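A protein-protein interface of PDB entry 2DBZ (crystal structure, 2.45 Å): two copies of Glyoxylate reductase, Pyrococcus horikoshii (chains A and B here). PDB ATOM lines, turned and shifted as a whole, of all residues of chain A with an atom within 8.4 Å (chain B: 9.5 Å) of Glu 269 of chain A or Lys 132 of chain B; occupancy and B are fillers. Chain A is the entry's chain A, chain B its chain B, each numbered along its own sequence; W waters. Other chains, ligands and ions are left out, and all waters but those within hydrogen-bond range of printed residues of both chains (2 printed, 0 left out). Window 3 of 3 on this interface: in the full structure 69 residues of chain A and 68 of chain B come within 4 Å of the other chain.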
ATOM      1  N   LYS A  32      29.004  19.445  -6.043  1.00  0.00           N
ATOM      2  CA  LYS A  32      28.141  19.043  -4.948  1.00  0.00           C
ATOM      3  C   LYS A  32      27.150  20.154  -4.729  1.00  0.00           C
ATOM      4  O   LYS A  32      27.397  21.302  -5.106  1.00  0.00           O
ATOM      5  CB  LYS A  32      28.938  18.792  -3.658  1.00  0.00           C
ATOM      6  CG  LYS A  32      28.096  18.243  -2.493  1.00  0.00           C
ATOM      7  CD  LYS A  32      28.891  18.128  -1.187  1.00  0.00           C
ATOM      8  CE  LYS A  32      29.989  17.077  -1.280  1.00  0.00           C
ATOM      9  NZ  LYS A  32      30.713  16.893   0.017  1.00  0.00           N
ATOM     10  N   ARG A 241       9.861   9.240  -8.054  1.00  0.00           N
ATOM     11  CA  ARG A 241      10.528   9.826  -6.869  1.00  0.00           C
ATOM     12  C   ARG A 241      10.750   8.713  -5.870  1.00  0.00           C
ATOM     13  O   ARG A 241       9.889   7.867  -5.691  1.00  0.00           O
ATOM     14  CB  ARG A 241       9.680  10.922  -6.236  1.00  0.00           C
ATOM     15  CG  ARG A 241       9.779  12.236  -6.965  1.00  0.00           C
ATOM     16  CD  ARG A 241      11.044  13.012  -6.558  1.00  0.00           C
ATOM     17  NE  ARG A 241      11.179  14.271  -7.309  1.00  0.00           N
ATOM     18  CZ  ARG A 241      11.731  14.355  -8.520  1.00  0.00           C
ATOM     19  NH1 ARG A 241      12.201  13.262  -9.113  1.00  0.00           N
ATOM     20  NH2 ARG A 241      11.805  15.518  -9.145  1.00  0.00           N
ATOM     21  N   GLY A 242      11.908   8.700  -5.234  1.00  0.00           N
ATOM     22  CA  GLY A 242      12.208   7.629  -4.301  1.00  0.00           C
ATOM     23  C   GLY A 242      11.155   7.316  -3.250  1.00  0.00           C
ATOM     24  O   GLY A 242      10.948   6.148  -2.913  1.00  0.00           O
ATOM     25  N   LYS A 243      10.471   8.347  -2.751  1.00  0.00           N
ATOM     26  CA  LYS A 243       9.494   8.189  -1.683  1.00  0.00           C
ATOM     27  C   LYS A 243       8.114   7.696  -2.080  1.00  0.00           C
ATOM     28  O   LYS A 243       7.239   7.542  -1.227  1.00  0.00           O
ATOM     29  CB  LYS A 243       9.382   9.499  -0.896  1.00  0.00           C
ATOM     30  CG  LYS A 243      10.595   9.779  -0.011  1.00  0.00           C
ATOM     31  CD  LYS A 243      10.564  11.212   0.517  1.00  0.00           C
ATOM     32  CE  LYS A 243      11.858  11.611   1.223  1.00  0.00           C
ATOM     33  NZ  LYS A 243      11.833  13.075   1.461  1.00  0.00           N
ATOM     34  N   THR A 247      10.960   1.747   0.623  1.00  0.00           N
ATOM     35  CA  THR A 247      12.152   0.923   0.413  1.00  0.00           C
ATOM     36  C   THR A 247      12.177  -0.349   1.251  1.00  0.00           C
ATOM     37  O   THR A 247      12.454  -1.435   0.732  1.00  0.00           O
ATOM     38  CB  THR A 247      13.440   1.697   0.724  1.00  0.00           C
ATOM     39  OG1 THR A 247      13.332   3.034   0.223  1.00  0.00           O
ATOM     40  CG2 THR A 247      14.639   0.987   0.089  1.00  0.00           C
ATOM     41  N   VAL A 266      15.448   6.364  -8.731  1.00  0.00           N
ATOM     42  CA  VAL A 266      15.317   7.338  -7.643  1.00  0.00           C
ATOM     43  C   VAL A 266      15.270   6.680  -6.263  1.00  0.00           C
ATOM     44  O   VAL A 266      14.949   5.498  -6.138  1.00  0.00           O
ATOM     45  CB  VAL A 266      14.083   8.228  -7.851  1.00  0.00           C
ATOM     46  CG1 VAL A 266      14.304   9.120  -9.061  1.00  0.00           C
ATOM     47  CG2 VAL A 266      12.864   7.367  -8.109  1.00  0.00           C
ATOM     48  N   PHE A 267      15.627   7.438  -5.234  1.00  0.00           N
ATOM     49  CA  PHE A 267      15.674   6.900  -3.871  1.00  0.00           C
ATOM     50  C   PHE A 267      15.159   7.897  -2.837  1.00  0.00           C
ATOM     51  O   PHE A 267      15.130   9.105  -3.087  1.00  0.00           O
ATOM     52  CB  PHE A 267      17.113   6.474  -3.571  1.00  0.00           C
ATOM     53  CG  PHE A 267      17.663   5.507  -4.580  1.00  0.00           C
ATOM     54  CD1 PHE A 267      17.631   4.138  -4.347  1.00  0.00           C
ATOM     55  CD2 PHE A 267      18.142   5.967  -5.797  1.00  0.00           C
ATOM     56  CE1 PHE A 267      18.067   3.236  -5.316  1.00  0.00           C
ATOM     57  CE2 PHE A 267      18.578   5.079  -6.777  1.00  0.00           C
ATOM     58  CZ  PHE A 267      18.541   3.709  -6.538  1.00  0.00           C
ATOM     59  N   GLU A 268      14.754   7.397  -1.675  1.00  0.00           N
ATOM     60  CA  GLU A 268      14.200   8.271  -0.636  1.00  0.00           C
ATOM     61  C   GLU A 268      15.214   9.302  -0.139  1.00  0.00           C
ATOM     62  O   GLU A 268      14.858  10.397   0.298  1.00  0.00           O
ATOM     63  CB  GLU A 268      13.647   7.428   0.521  1.00  0.00           C
ATOM     64  CG  GLU A 268      12.636   6.367   0.068  1.00  0.00           C
ATOM     65  CD  GLU A 268      11.742   5.886   1.198  1.00  0.00           C
ATOM     66  OE1 GLU A 268      10.904   6.687   1.672  1.00  0.00           O
ATOM     67  OE2 GLU A 268      11.882   4.715   1.616  1.00  0.00           O
ATOM     68  N   GLU A 269      16.482   8.950  -0.254  1.00  0.00           N
ATOM     69  CA  GLU A 269      17.564   9.824   0.147  1.00  0.00           C
ATOM     70  C   GLU A 269      18.614   9.748  -0.971  1.00  0.00           C
ATOM     71  O   GLU A 269      18.958   8.651  -1.425  1.00  0.00           O
ATOM     72  CB  GLU A 269      18.132   9.321   1.469  1.00  0.00           C
ATOM     73  CG  GLU A 269      19.005  10.280   2.209  1.00  0.00           C
ATOM     74  CD  GLU A 269      19.549   9.655   3.486  1.00  0.00           C
ATOM     75  OE1 GLU A 269      18.741   9.039   4.224  1.00  0.00           O
ATOM     76  OE2 GLU A 269      20.773   9.778   3.749  1.00  0.00           O
ATOM     77  N   GLU A 270      19.110  10.903  -1.421  1.00  0.00           N
ATOM     78  CA  GLU A 270      20.113  10.946  -2.490  1.00  0.00           C
ATOM     79  C   GLU A 270      21.310  11.848  -2.164  1.00  0.00           C
ATOM     80  O   GLU A 270      21.125  12.992  -1.746  1.00  0.00           O
ATOM     81  CB  GLU A 270      19.454  11.420  -3.791  1.00  0.00           C
ATOM     82  CG  GLU A 270      18.138  10.727  -4.037  1.00  0.00           C
ATOM     83  CD  GLU A 270      17.536  11.025  -5.387  1.00  0.00           C
ATOM     84  OE1 GLU A 270      17.683  12.159  -5.913  1.00  0.00           O
ATOM     85  OE2 GLU A 270      16.888  10.105  -5.912  1.00  0.00           O
ATOM     86  N   PRO A 271      22.554  11.350  -2.375  1.00  0.00           N
ATOM     87  CA  PRO A 271      22.779   9.998  -2.894  1.00  0.00           C
ATOM     88  C   PRO A 271      22.328   8.988  -1.867  1.00  0.00           C
ATOM     89  O   PRO A 271      21.998   9.348  -0.732  1.00  0.00           O
ATOM     90  CB  PRO A 271      24.290   9.965  -3.174  1.00  0.00           C
ATOM     91  CG  PRO A 271      24.848  10.879  -2.169  1.00  0.00           C
ATOM     92  CD  PRO A 271      23.833  12.034  -2.136  1.00  0.00           C
ATOM     93  N   TYR A 272      22.350   7.721  -2.247  1.00  0.00           N
ATOM     94  CA  TYR A 272      21.842   6.679  -1.373  1.00  0.00           C
ATOM     95  C   TYR A 272      22.737   5.453  -1.254  1.00  0.00           C
ATOM     96  O   TYR A 272      23.434   5.072  -2.203  1.00  0.00           O
ATOM     97  CB  TYR A 272      20.472   6.268  -1.925  1.00  0.00           C
ATOM     98  CG  TYR A 272      19.657   5.296  -1.102  1.00  0.00           C
ATOM     99  CD1 TYR A 272      18.956   5.721   0.023  1.00  0.00           C
ATOM    100  CD2 TYR A 272      19.516   3.964  -1.497  1.00  0.00           C
ATOM    101  CE1 TYR A 272      18.119   4.847   0.734  1.00  0.00           C
ATOM    102  CE2 TYR A 272      18.689   3.087  -0.796  1.00  0.00           C
ATOM    103  CZ  TYR A 272      17.988   3.539   0.315  1.00  0.00           C
ATOM    104  OH  TYR A 272      17.122   2.694   0.966  1.00  0.00           O
ATOM    105  N   TYR A 273      22.726   4.848  -0.075  1.00  0.00           N
ATOM    106  CA  TYR A 273      23.465   3.612   0.135  1.00  0.00           C
ATOM    107  C   TYR A 273      22.585   2.734   1.028  1.00  0.00           C
ATOM    108  O   TYR A 273      21.937   3.222   1.948  1.00  0.00           O
ATOM    109  CB  TYR A 273      24.833   3.837   0.795  1.00  0.00           C
ATOM    110  CG  TYR A 273      25.611   2.542   0.883  1.00  0.00           C
ATOM    111  CD1 TYR A 273      26.091   1.922  -0.272  1.00  0.00           C
ATOM    112  CD2 TYR A 273      25.778   1.879   2.101  1.00  0.00           C
ATOM    113  CE1 TYR A 273      26.718   0.667  -0.224  1.00  0.00           C
ATOM    114  CE2 TYR A 273      26.410   0.606   2.162  1.00  0.00           C
ATOM    115  CZ  TYR A 273      26.873   0.014   0.988  1.00  0.00           C
ATOM    116  OH  TYR A 273      27.484  -1.226   0.997  1.00  0.00           O
ATOM    117  N   ASN A 274      22.552   1.443   0.747  1.00  0.00           N
ATOM    118  CA  ASN A 274      21.726   0.519   1.514  1.00  0.00           C
ATOM    119  C   ASN A 274      22.310  -0.833   1.195  1.00  0.00           C
ATOM    120  O   ASN A 274      22.079  -1.344   0.116  1.00  0.00           O
ATOM    121  CB  ASN A 274      20.279   0.587   1.020  1.00  0.00           C
ATOM    122  CG  ASN A 274      19.380  -0.420   1.705  1.00  0.00           C
ATOM    123  OD1 ASN A 274      19.775  -1.568   1.943  1.00  0.00           O
ATOM    124  ND2 ASN A 274      18.149  -0.002   2.009  1.00  0.00           N
ATOM    125  N   PHE A 278      21.405  -3.297  -2.205  1.00  0.00           N
ATOM    126  CA  PHE A 278      22.560  -3.462  -3.086  1.00  0.00           C
ATOM    127  C   PHE A 278      23.220  -4.861  -3.151  1.00  0.00           C
ATOM    128  O   PHE A 278      24.037  -5.127  -4.037  1.00  0.00           O
ATOM    129  CB  PHE A 278      23.618  -2.416  -2.717  1.00  0.00           C
ATOM    130  CG  PHE A 278      23.142  -0.990  -2.847  1.00  0.00           C
ATOM    131  CD1 PHE A 278      21.787  -0.698  -3.039  1.00  0.00           C
ATOM    132  CD2 PHE A 278      24.035   0.067  -2.677  1.00  0.00           C
ATOM    133  CE1 PHE A 278      21.326   0.618  -3.047  1.00  0.00           C
ATOM    134  CE2 PHE A 278      23.586   1.390  -2.684  1.00  0.00           C
ATOM    135  CZ  PHE A 278      22.230   1.665  -2.867  1.00  0.00           C
ATOM    136  N   PRO A 287      21.833   6.227 -10.678  1.00  0.00           N
ATOM    137  CA  PRO A 287      21.862   7.480  -9.904  1.00  0.00           C
ATOM    138  C   PRO A 287      21.007   8.661 -10.361  1.00  0.00           C
ATOM    139  O   PRO A 287      21.515   9.742 -10.641  1.00  0.00           O
ATOM    140  CB  PRO A 287      23.352   7.819  -9.869  1.00  0.00           C
ATOM    141  CG  PRO A 287      23.846   7.286 -11.210  1.00  0.00           C
ATOM    142  CD  PRO A 287      23.150   5.940 -11.283  1.00  0.00           C
ATOM    143  N   HIS A 288      19.701   8.460 -10.397  1.00  0.00           N
ATOM    144  CA  HIS A 288      18.783   9.510 -10.819  1.00  0.00           C
ATOM    145  C   HIS A 288      19.237  10.209 -12.109  1.00  0.00           C
ATOM    146  O   HIS A 288      19.422  11.432 -12.146  1.00  0.00           O
ATOM    147  CB  HIS A 288      18.597  10.524  -9.679  1.00  0.00           C
ATOM    148  CG  HIS A 288      17.347  11.346  -9.803  1.00  0.00           C
ATOM    149  ND1 HIS A 288      16.807  12.051  -8.747  1.00  0.00           N
ATOM    150  CD2 HIS A 288      16.582  11.638 -10.884  1.00  0.00           C
ATOM    151  CE1 HIS A 288      15.772  12.750  -9.178  1.00  0.00           C
ATOM    152  NE2 HIS A 288      15.615  12.518 -10.471  1.00  0.00           N
ATOM    153  N   GLY B 122      26.243   3.339 -14.370  1.00  0.00           N
ATOM    154  CA  GLY B 122      25.534   4.039 -13.316  1.00  0.00           C
ATOM    155  C   GLY B 122      25.213   3.097 -12.168  1.00  0.00           C
ATOM    156  O   GLY B 122      25.191   3.503 -11.004  1.00  0.00           O
ATOM    157  N   ARG B 124      26.984   0.368 -11.249  1.00  0.00           N
ATOM    158  CA  ARG B 124      28.211   0.109 -10.531  1.00  0.00           C
ATOM    159  C   ARG B 124      28.452   1.284  -9.561  1.00  0.00           C
ATOM    160  O   ARG B 124      28.761   1.075  -8.392  1.00  0.00           O
ATOM    161  CB  ARG B 124      29.360  -0.008 -11.519  1.00  0.00           C
ATOM    162  CG  ARG B 124      30.517  -0.870 -11.035  1.00  0.00           C
ATOM    163  CD  ARG B 124      31.513  -1.030 -12.162  1.00  0.00           C
ATOM    164  NE  ARG B 124      30.796  -1.161 -13.433  1.00  0.00           N
ATOM    165  CZ  ARG B 124      31.378  -1.291 -14.621  1.00  0.00           C
ATOM    166  NH1 ARG B 124      32.705  -1.319 -14.712  1.00  0.00           N
ATOM    167  NH2 ARG B 124      30.630  -1.368 -15.720  1.00  0.00           N
ATOM    168  N   PHE B 125      28.259   2.505 -10.063  1.00  0.00           N
ATOM    169  CA  PHE B 125      28.437   3.747  -9.314  1.00  0.00           C
ATOM    170  C   PHE B 125      27.597   3.796  -8.045  1.00  0.00           C
ATOM    171  O   PHE B 125      28.076   4.242  -6.981  1.00  0.00           O
ATOM    172  CB  PHE B 125      28.058   4.930 -10.206  1.00  0.00           C
ATOM    173  CG  PHE B 125      28.376   6.295  -9.616  1.00  0.00           C
ATOM    174  CD1 PHE B 125      29.692   6.683  -9.374  1.00  0.00           C
ATOM    175  CD2 PHE B 125      27.362   7.225  -9.398  1.00  0.00           C
ATOM    176  CE1 PHE B 125      29.996   7.983  -8.934  1.00  0.00           C
ATOM    177  CE2 PHE B 125      27.652   8.531  -8.957  1.00  0.00           C
ATOM    178  CZ  PHE B 125      28.974   8.908  -8.729  1.00  0.00           C
ATOM    179  N   VAL B 126      26.341   3.357  -8.161  1.00  0.00           N
ATOM    180  CA  VAL B 126      25.435   3.359  -7.022  1.00  0.00           C
ATOM    181  C   VAL B 126      25.733   2.189  -6.081  1.00  0.00           C
ATOM    182  O   VAL B 126      25.979   2.366  -4.891  1.00  0.00           O
ATOM    183  CB  VAL B 126      23.965   3.243  -7.470  1.00  0.00           C
ATOM    184  CG1 VAL B 126      23.059   3.151  -6.249  1.00  0.00           C
ATOM    185  CG2 VAL B 126      23.574   4.440  -8.301  1.00  0.00           C
ATOM    186  N   ARG B 127      25.717   0.992  -6.640  1.00  0.00           N
ATOM    187  CA  ARG B 127      25.938  -0.238  -5.893  1.00  0.00           C
ATOM    188  C   ARG B 127      27.253  -0.308  -5.128  1.00  0.00           C
ATOM    189  O   ARG B 127      27.314  -0.919  -4.067  1.00  0.00           O
ATOM    190  CB  ARG B 127      25.852  -1.421  -6.858  1.00  0.00           C
ATOM    191  CG  ARG B 127      25.756  -2.778  -6.215  1.00  0.00           C
ATOM    192  CD  ARG B 127      25.675  -3.834  -7.303  1.00  0.00           C
ATOM    193  NE  ARG B 127      24.534  -3.668  -8.217  1.00  0.00           N
ATOM    194  CZ  ARG B 127      23.288  -4.089  -7.978  1.00  0.00           C
ATOM    195  NH1 ARG B 127      22.994  -4.708  -6.843  1.00  0.00           N
ATOM    196  NH2 ARG B 127      22.344  -3.927  -8.899  1.00  0.00           N
ATOM    197  N   SER B 128      28.301   0.309  -5.667  1.00  0.00           N
ATOM    198  CA  SER B 128      29.614   0.269  -5.032  1.00  0.00           C
ATOM    199  C   SER B 128      29.720   1.247  -3.876  1.00  0.00           C
ATOM    200  O   SER B 128      30.680   1.204  -3.110  1.00  0.00           O
ATOM    201  CB  SER B 128      30.703   0.583  -6.050  1.00  0.00           C
ATOM    202  OG  SER B 128      30.598   1.937  -6.429  1.00  0.00           O
ATOM    203  N   GLY B 129      28.739   2.134  -3.764  1.00  0.00           N
ATOM    204  CA  GLY B 129      28.738   3.105  -2.687  1.00  0.00           C
ATOM    205  C   GLY B 129      29.424   4.400  -3.078  1.00  0.00           C
ATOM    206  O   GLY B 129      29.375   5.403  -2.348  1.00  0.00           O
ATOM    207  N   GLU B 130      30.060   4.374  -4.243  1.00  0.00           N
ATOM    208  CA  GLU B 130      30.772   5.526  -4.762  1.00  0.00           C
ATOM    209  C   GLU B 130      29.888   6.765  -4.873  1.00  0.00           C
ATOM    210  O   GLU B 130      30.333   7.880  -4.595  1.00  0.00           O
ATOM    211  CB  GLU B 130      31.369   5.185  -6.131  1.00  0.00           C
ATOM    212  CG  GLU B 130      32.702   5.853  -6.388  1.00  0.00           C
ATOM    213  CD  GLU B 130      33.731   5.492  -5.324  1.00  0.00           C
ATOM    214  OE1 GLU B 130      34.058   4.289  -5.184  1.00  0.00           O
ATOM    215  OE2 GLU B 130      34.205   6.411  -4.626  1.00  0.00           O
ATOM    216  N   TRP B 131      28.638   6.571  -5.282  1.00  0.00           N
ATOM    217  CA  TRP B 131      27.712   7.684  -5.436  1.00  0.00           C
ATOM    218  C   TRP B 131      27.472   8.360  -4.097  1.00  0.00           C
ATOM    219  O   TRP B 131      27.433   9.591  -4.013  1.00  0.00           O
ATOM    220  CB  TRP B 131      26.383   7.186  -6.036  1.00  0.00           C
ATOM    221  CG  TRP B 131      25.329   8.253  -6.248  1.00  0.00           C
ATOM    222  CD1 TRP B 131      25.535   9.564  -6.619  1.00  0.00           C
ATOM    223  CD2 TRP B 131      23.901   8.089  -6.154  1.00  0.00           C
ATOM    224  NE1 TRP B 131      24.329  10.214  -6.755  1.00  0.00           N
ATOM    225  CE2 TRP B 131      23.312   9.335  -6.475  1.00  0.00           C
ATOM    226  CE3 TRP B 131      23.062   7.007  -5.831  1.00  0.00           C
ATOM    227  CZ2 TRP B 131      21.918   9.530  -6.479  1.00  0.00           C
ATOM    228  CZ3 TRP B 131      21.676   7.202  -5.837  1.00  0.00           C
ATOM    229  CH2 TRP B 131      21.122   8.455  -6.159  1.00  0.00           C
ATOM    230  N   LYS B 132      27.301   7.553  -3.056  1.00  0.00           N
ATOM    231  CA  LYS B 132      27.063   8.070  -1.703  1.00  0.00           C
ATOM    232  C   LYS B 132      28.321   8.806  -1.211  1.00  0.00           C
ATOM    233  O   LYS B 132      28.249   9.914  -0.685  1.00  0.00           O
ATOM    234  CB  LYS B 132      26.726   6.899  -0.767  1.00  0.00           C
ATOM    235  CG  LYS B 132      26.612   7.244   0.708  1.00  0.00           C
ATOM    236  CD  LYS B 132      25.410   8.118   1.006  1.00  0.00           C
ATOM    237  CE  LYS B 132      25.331   8.434   2.503  1.00  0.00           C
ATOM    238  NZ  LYS B 132      24.027   9.052   2.900  1.00  0.00           N
ATOM    239  N   LYS B 133      29.467   8.164  -1.407  1.00  0.00           N
ATOM    240  CA  LYS B 133      30.766   8.694  -1.025  1.00  0.00           C
ATOM    241  C   LYS B 133      30.979  10.101  -1.582  1.00  0.00           C
ATOM    242  O   LYS B 133      31.337  11.016  -0.842  1.00  0.00           O
ATOM    243  CB  LYS B 133      31.854   7.738  -1.522  1.00  0.00           C
ATOM    244  CG  LYS B 133      33.274   8.178  -1.243  1.00  0.00           C
ATOM    245  CD  LYS B 133      34.277   7.159  -1.794  1.00  0.00           C
ATOM    246  CE  LYS B 133      35.720   7.678  -1.743  1.00  0.00           C
ATOM    247  NZ  LYS B 133      36.706   6.766  -2.415  1.00  0.00           N
ATOM    248  N   ARG B 134      30.745  10.271  -2.882  1.00  0.00           N
ATOM    249  CA  ARG B 134      30.900  11.562  -3.561  1.00  0.00           C
ATOM    250  C   ARG B 134      30.065  12.704  -2.984  1.00  0.00           C
ATOM    251  O   ARG B 134      30.349  13.878  -3.241  1.00  0.00           O
ATOM    252  CB  ARG B 134      30.554  11.413  -5.043  1.00  0.00           C
ATOM    253  CG  ARG B 134      31.724  11.068  -5.921  1.00  0.00           C
ATOM    254  CD  ARG B 134      32.065  12.238  -6.833  1.00  0.00           C
ATOM    255  NE  ARG B 134      32.568  11.759  -8.117  1.00  0.00           N
ATOM    256  CZ  ARG B 134      32.721  12.523  -9.194  1.00  0.00           C
ATOM    257  NH1 ARG B 134      32.419  13.813  -9.146  1.00  0.00           N
ATOM    258  NH2 ARG B 134      33.147  11.989 -10.332  1.00  0.00           N
ATOM    259  N   GLY B 135      29.017  12.378  -2.239  1.00  0.00           N
ATOM    260  CA  GLY B 135      28.210  13.434  -1.654  1.00  0.00           C
ATOM    261  C   GLY B 135      27.381  14.240  -2.630  1.00  0.00           C
ATOM    262  O   GLY B 135      26.732  15.219  -2.237  1.00  0.00           O
ATOM    263  N   VAL B 136      27.401  13.848  -3.901  1.00  0.00           N
ATOM    264  CA  VAL B 136      26.611  14.547  -4.912  1.00  0.00           C
ATOM    265  C   VAL B 136      25.365  13.751  -5.266  1.00  0.00           C
ATOM    266  O   VAL B 136      25.441  12.573  -5.639  1.00  0.00           O
ATOM    267  CB  VAL B 136      27.373  14.766  -6.213  1.00  0.00           C
ATOM    268  CG1 VAL B 136      26.481  15.534  -7.178  1.00  0.00           C
ATOM    269  CG2 VAL B 136      28.671  15.515  -5.952  1.00  0.00           C
ATOM    270  N   ALA B 137      24.223  14.420  -5.178  1.00  0.00           N
ATOM    271  CA  ALA B 137      22.943  13.798  -5.466  1.00  0.00           C
ATOM    272  C   ALA B 137      22.559  13.770  -6.949  1.00  0.00           C
ATOM    273  O   ALA B 137      22.426  12.702  -7.565  1.00  0.00           O
ATOM    274  CB  ALA B 137      21.870  14.506  -4.680  1.00  0.00           C
ATOM    275  N   TRP B 138      22.388  14.958  -7.513  1.00  0.00           N
ATOM    276  CA  TRP B 138      21.970  15.109  -8.893  1.00  0.00           C
ATOM    277  C   TRP B 138      22.806  16.222  -9.495  1.00  0.00           C
ATOM    278  O   TRP B 138      23.001  17.259  -8.867  1.00  0.00           O
ATOM    279  CB  TRP B 138      20.485  15.506  -8.910  1.00  0.00           C
ATOM    280  CG  TRP B 138      19.819  15.503 -10.251  1.00  0.00           C
ATOM    281  CD1 TRP B 138      19.131  14.469 -10.825  1.00  0.00           C
ATOM    282  CD2 TRP B 138      19.785  16.578 -11.194  1.00  0.00           C
ATOM    283  NE1 TRP B 138      18.665  14.840 -12.069  1.00  0.00           N
ATOM    284  CE2 TRP B 138      19.049  16.129 -12.318  1.00  0.00           C
ATOM    285  CE3 TRP B 138      20.298  17.879 -11.199  1.00  0.00           C
ATOM    286  CZ2 TRP B 138      18.818  16.934 -13.434  1.00  0.00           C
ATOM    287  CZ3 TRP B 138      20.068  18.682 -12.309  1.00  0.00           C
ATOM    288  CH2 TRP B 138      19.338  18.204 -13.415  1.00  0.00           C
ATOM    289  N   TRP B 142      25.916  14.952 -15.359  1.00  0.00           N
ATOM    290  CA  TRP B 142      26.355  13.596 -15.004  1.00  0.00           C
ATOM    291  C   TRP B 142      25.719  12.479 -15.861  1.00  0.00           C
ATOM    292  O   TRP B 142      24.517  12.499 -16.172  1.00  0.00           O
ATOM    293  CB  TRP B 142      26.089  13.319 -13.506  1.00  0.00           C
ATOM    294  CG  TRP B 142      27.185  13.811 -12.580  1.00  0.00           C
ATOM    295  CD1 TRP B 142      28.107  14.788 -12.843  1.00  0.00           C
ATOM    296  CD2 TRP B 142      27.447  13.367 -11.245  1.00  0.00           C
ATOM    297  NE1 TRP B 142      28.923  14.973 -11.761  1.00  0.00           N
ATOM    298  CE2 TRP B 142      28.544  14.116 -10.763  1.00  0.00           C
ATOM    299  CE3 TRP B 142      26.865  12.407 -10.408  1.00  0.00           C
ATOM    300  CZ2 TRP B 142      29.070  13.934  -9.477  1.00  0.00           C
ATOM    301  CZ3 TRP B 142      27.388  12.227  -9.135  1.00  0.00           C
ATOM    302  CH2 TRP B 142      28.480  12.987  -8.680  1.00  0.00           C
HETATM  303  O   HOH W   1      17.986  12.778 -14.000  1.00  0.00           O
HETATM  304  O   HOH W   2      23.234  11.333  -9.845  1.00  0.00           O
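Among the printed residues, merely in contact across the chains: Pro 287 of chain A with Gly 122 of chain B (3.2 Å), Pro 271 of chain A with Trp 131 of chain B (3.3 Å), Lys 32 of chain A with Gly 135 of chain B (3.3 Å), Pro 287 of chain A with Val 126 of chain B (3.4 Å), Glu 270 of chain A with Ala 137 of chain B (3.4 Å), Phe 278 of chain A with Val 126 of chain B (3.4 Å), Pro 271 of chain A with Lys 132 of chain B (3.6 Å), Tyr 272 of chain A with Trp 131 of chain B (3.7 Å), Lys 32 of chain A with Val 136 of chain B (3.7 Å), Pro 287 of chain A with Trp 131 of chain B (3.7 Å), Phe 267 of chain A with Trp 131 of chain B (3.7 Å), Pro 271 of chain A with Val 136 of chain B (3.8 Å), Lys 32 of chain A with Arg 134 of chain B (3.8 Å), Tyr 273 of chain A with Gly 129 of chain B (3.8 Å), Tyr 273 of chain A with Lys 132 of chain B (3.8 Å), Pro 271 of chain A with Ala 137 of chain B (3.9 Å) and Pro 287 of chain A with Phe 125 of chain B (3.96 Å).
The side-chain carboxylate (OE2) of Glu 269 of chain A is in salt-bridge range of the side-chain amino group (NZ) of Lys 132 of chain B (3.4 Å).
O of His 288 of chain A sits close to NE1 of Trp 138 of chain B, 3.5 Å away.
The backbone carbonyl oxygen (O) of Phe 278 of chain A is in hydrogen-bond range of the guanidinium group (NH1) of Arg 127 of chain B.
Water W2 lies within hydrogen-bond range of the backbone carbonyl oxygen (O) of Pro 287 of chain A (2.5 Å), the backbone carbonyl oxygen (O) of Ala 137 of chain B (2.8 Å) and the indole nitrogen (NE1) of Trp 131 of chain B (3.5 Å).
Water W1 bridges O of His 288 of chain A (2.7 Å) and NE1 of Trp 138 of chain B (2.9 Å).
ND1 of His 288 of chain A lies within hydrogen-bond range of OE1 of Glu 270 of chain A (3.0 Å).
The side-chain hydroxyl (OG) of Ser 128 of chain B lies within hydrogen-bond range of the backbone carbonyl oxygen (O) of Phe 125 of chain B, 3.5 Å away.
The indole nitrogen (NE1) of Trp 131 of chain B sits at hydrogen-bond distance from the backbone carbonyl oxygen (O) of Ala 137 of chain B (3.2 Å).
N of Trp 131 of chain B sits at hydrogen-bond distance from O of Phe 125 of chain B.
The backbone carbonyl oxygen (O) of Val 136 of chain B lies within hydrogen-bond range of the indole nitrogen (NE1) of Trp 131 of chain B, at 2.8 Å.
Of the 17 printed residues of chain A, 10 touch a printed residue of chain B.
Hydrophobic or aromatic side chains of chain A within 4 Å of the printed part of chain B: Phe 267, Pro 271, Tyr 273, Phe 278, Pro 287 and His 288.
Along chain A the printed residues that touch a printed residue of chain B span positions 32 to 288.
Among the printed residues, Asp or Glu carboxylates within 4 Å of a Lys or Arg side-chain nitrogen of the other chain: Glu 269 of chain A with Lys 132 of chain B (3.4 Å).
No position is printed for both chains.
Thr 247 of chain A touches none of the printed residues of chain B.
Of the printed residues of chain B, Tyr 272 of chain A touches Trp 131 (3.7 Å).
Printed residues of chain B within 4 Å of Tyr 273 of chain A: Gly 129 (3.8 Å) and Lys 132 (3.8 Å).
Ser 128 of chain B touches none of the printed residues of chain A.
Printed residues of chain A within 4 Å of Trp 131 of chain B: Phe 267, Pro 271, Tyr 272 and Pro 287.
Of chain A, only Glu 269, Pro 271 and Tyr 273 come within 4 Å of Lys 132 of chain B.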
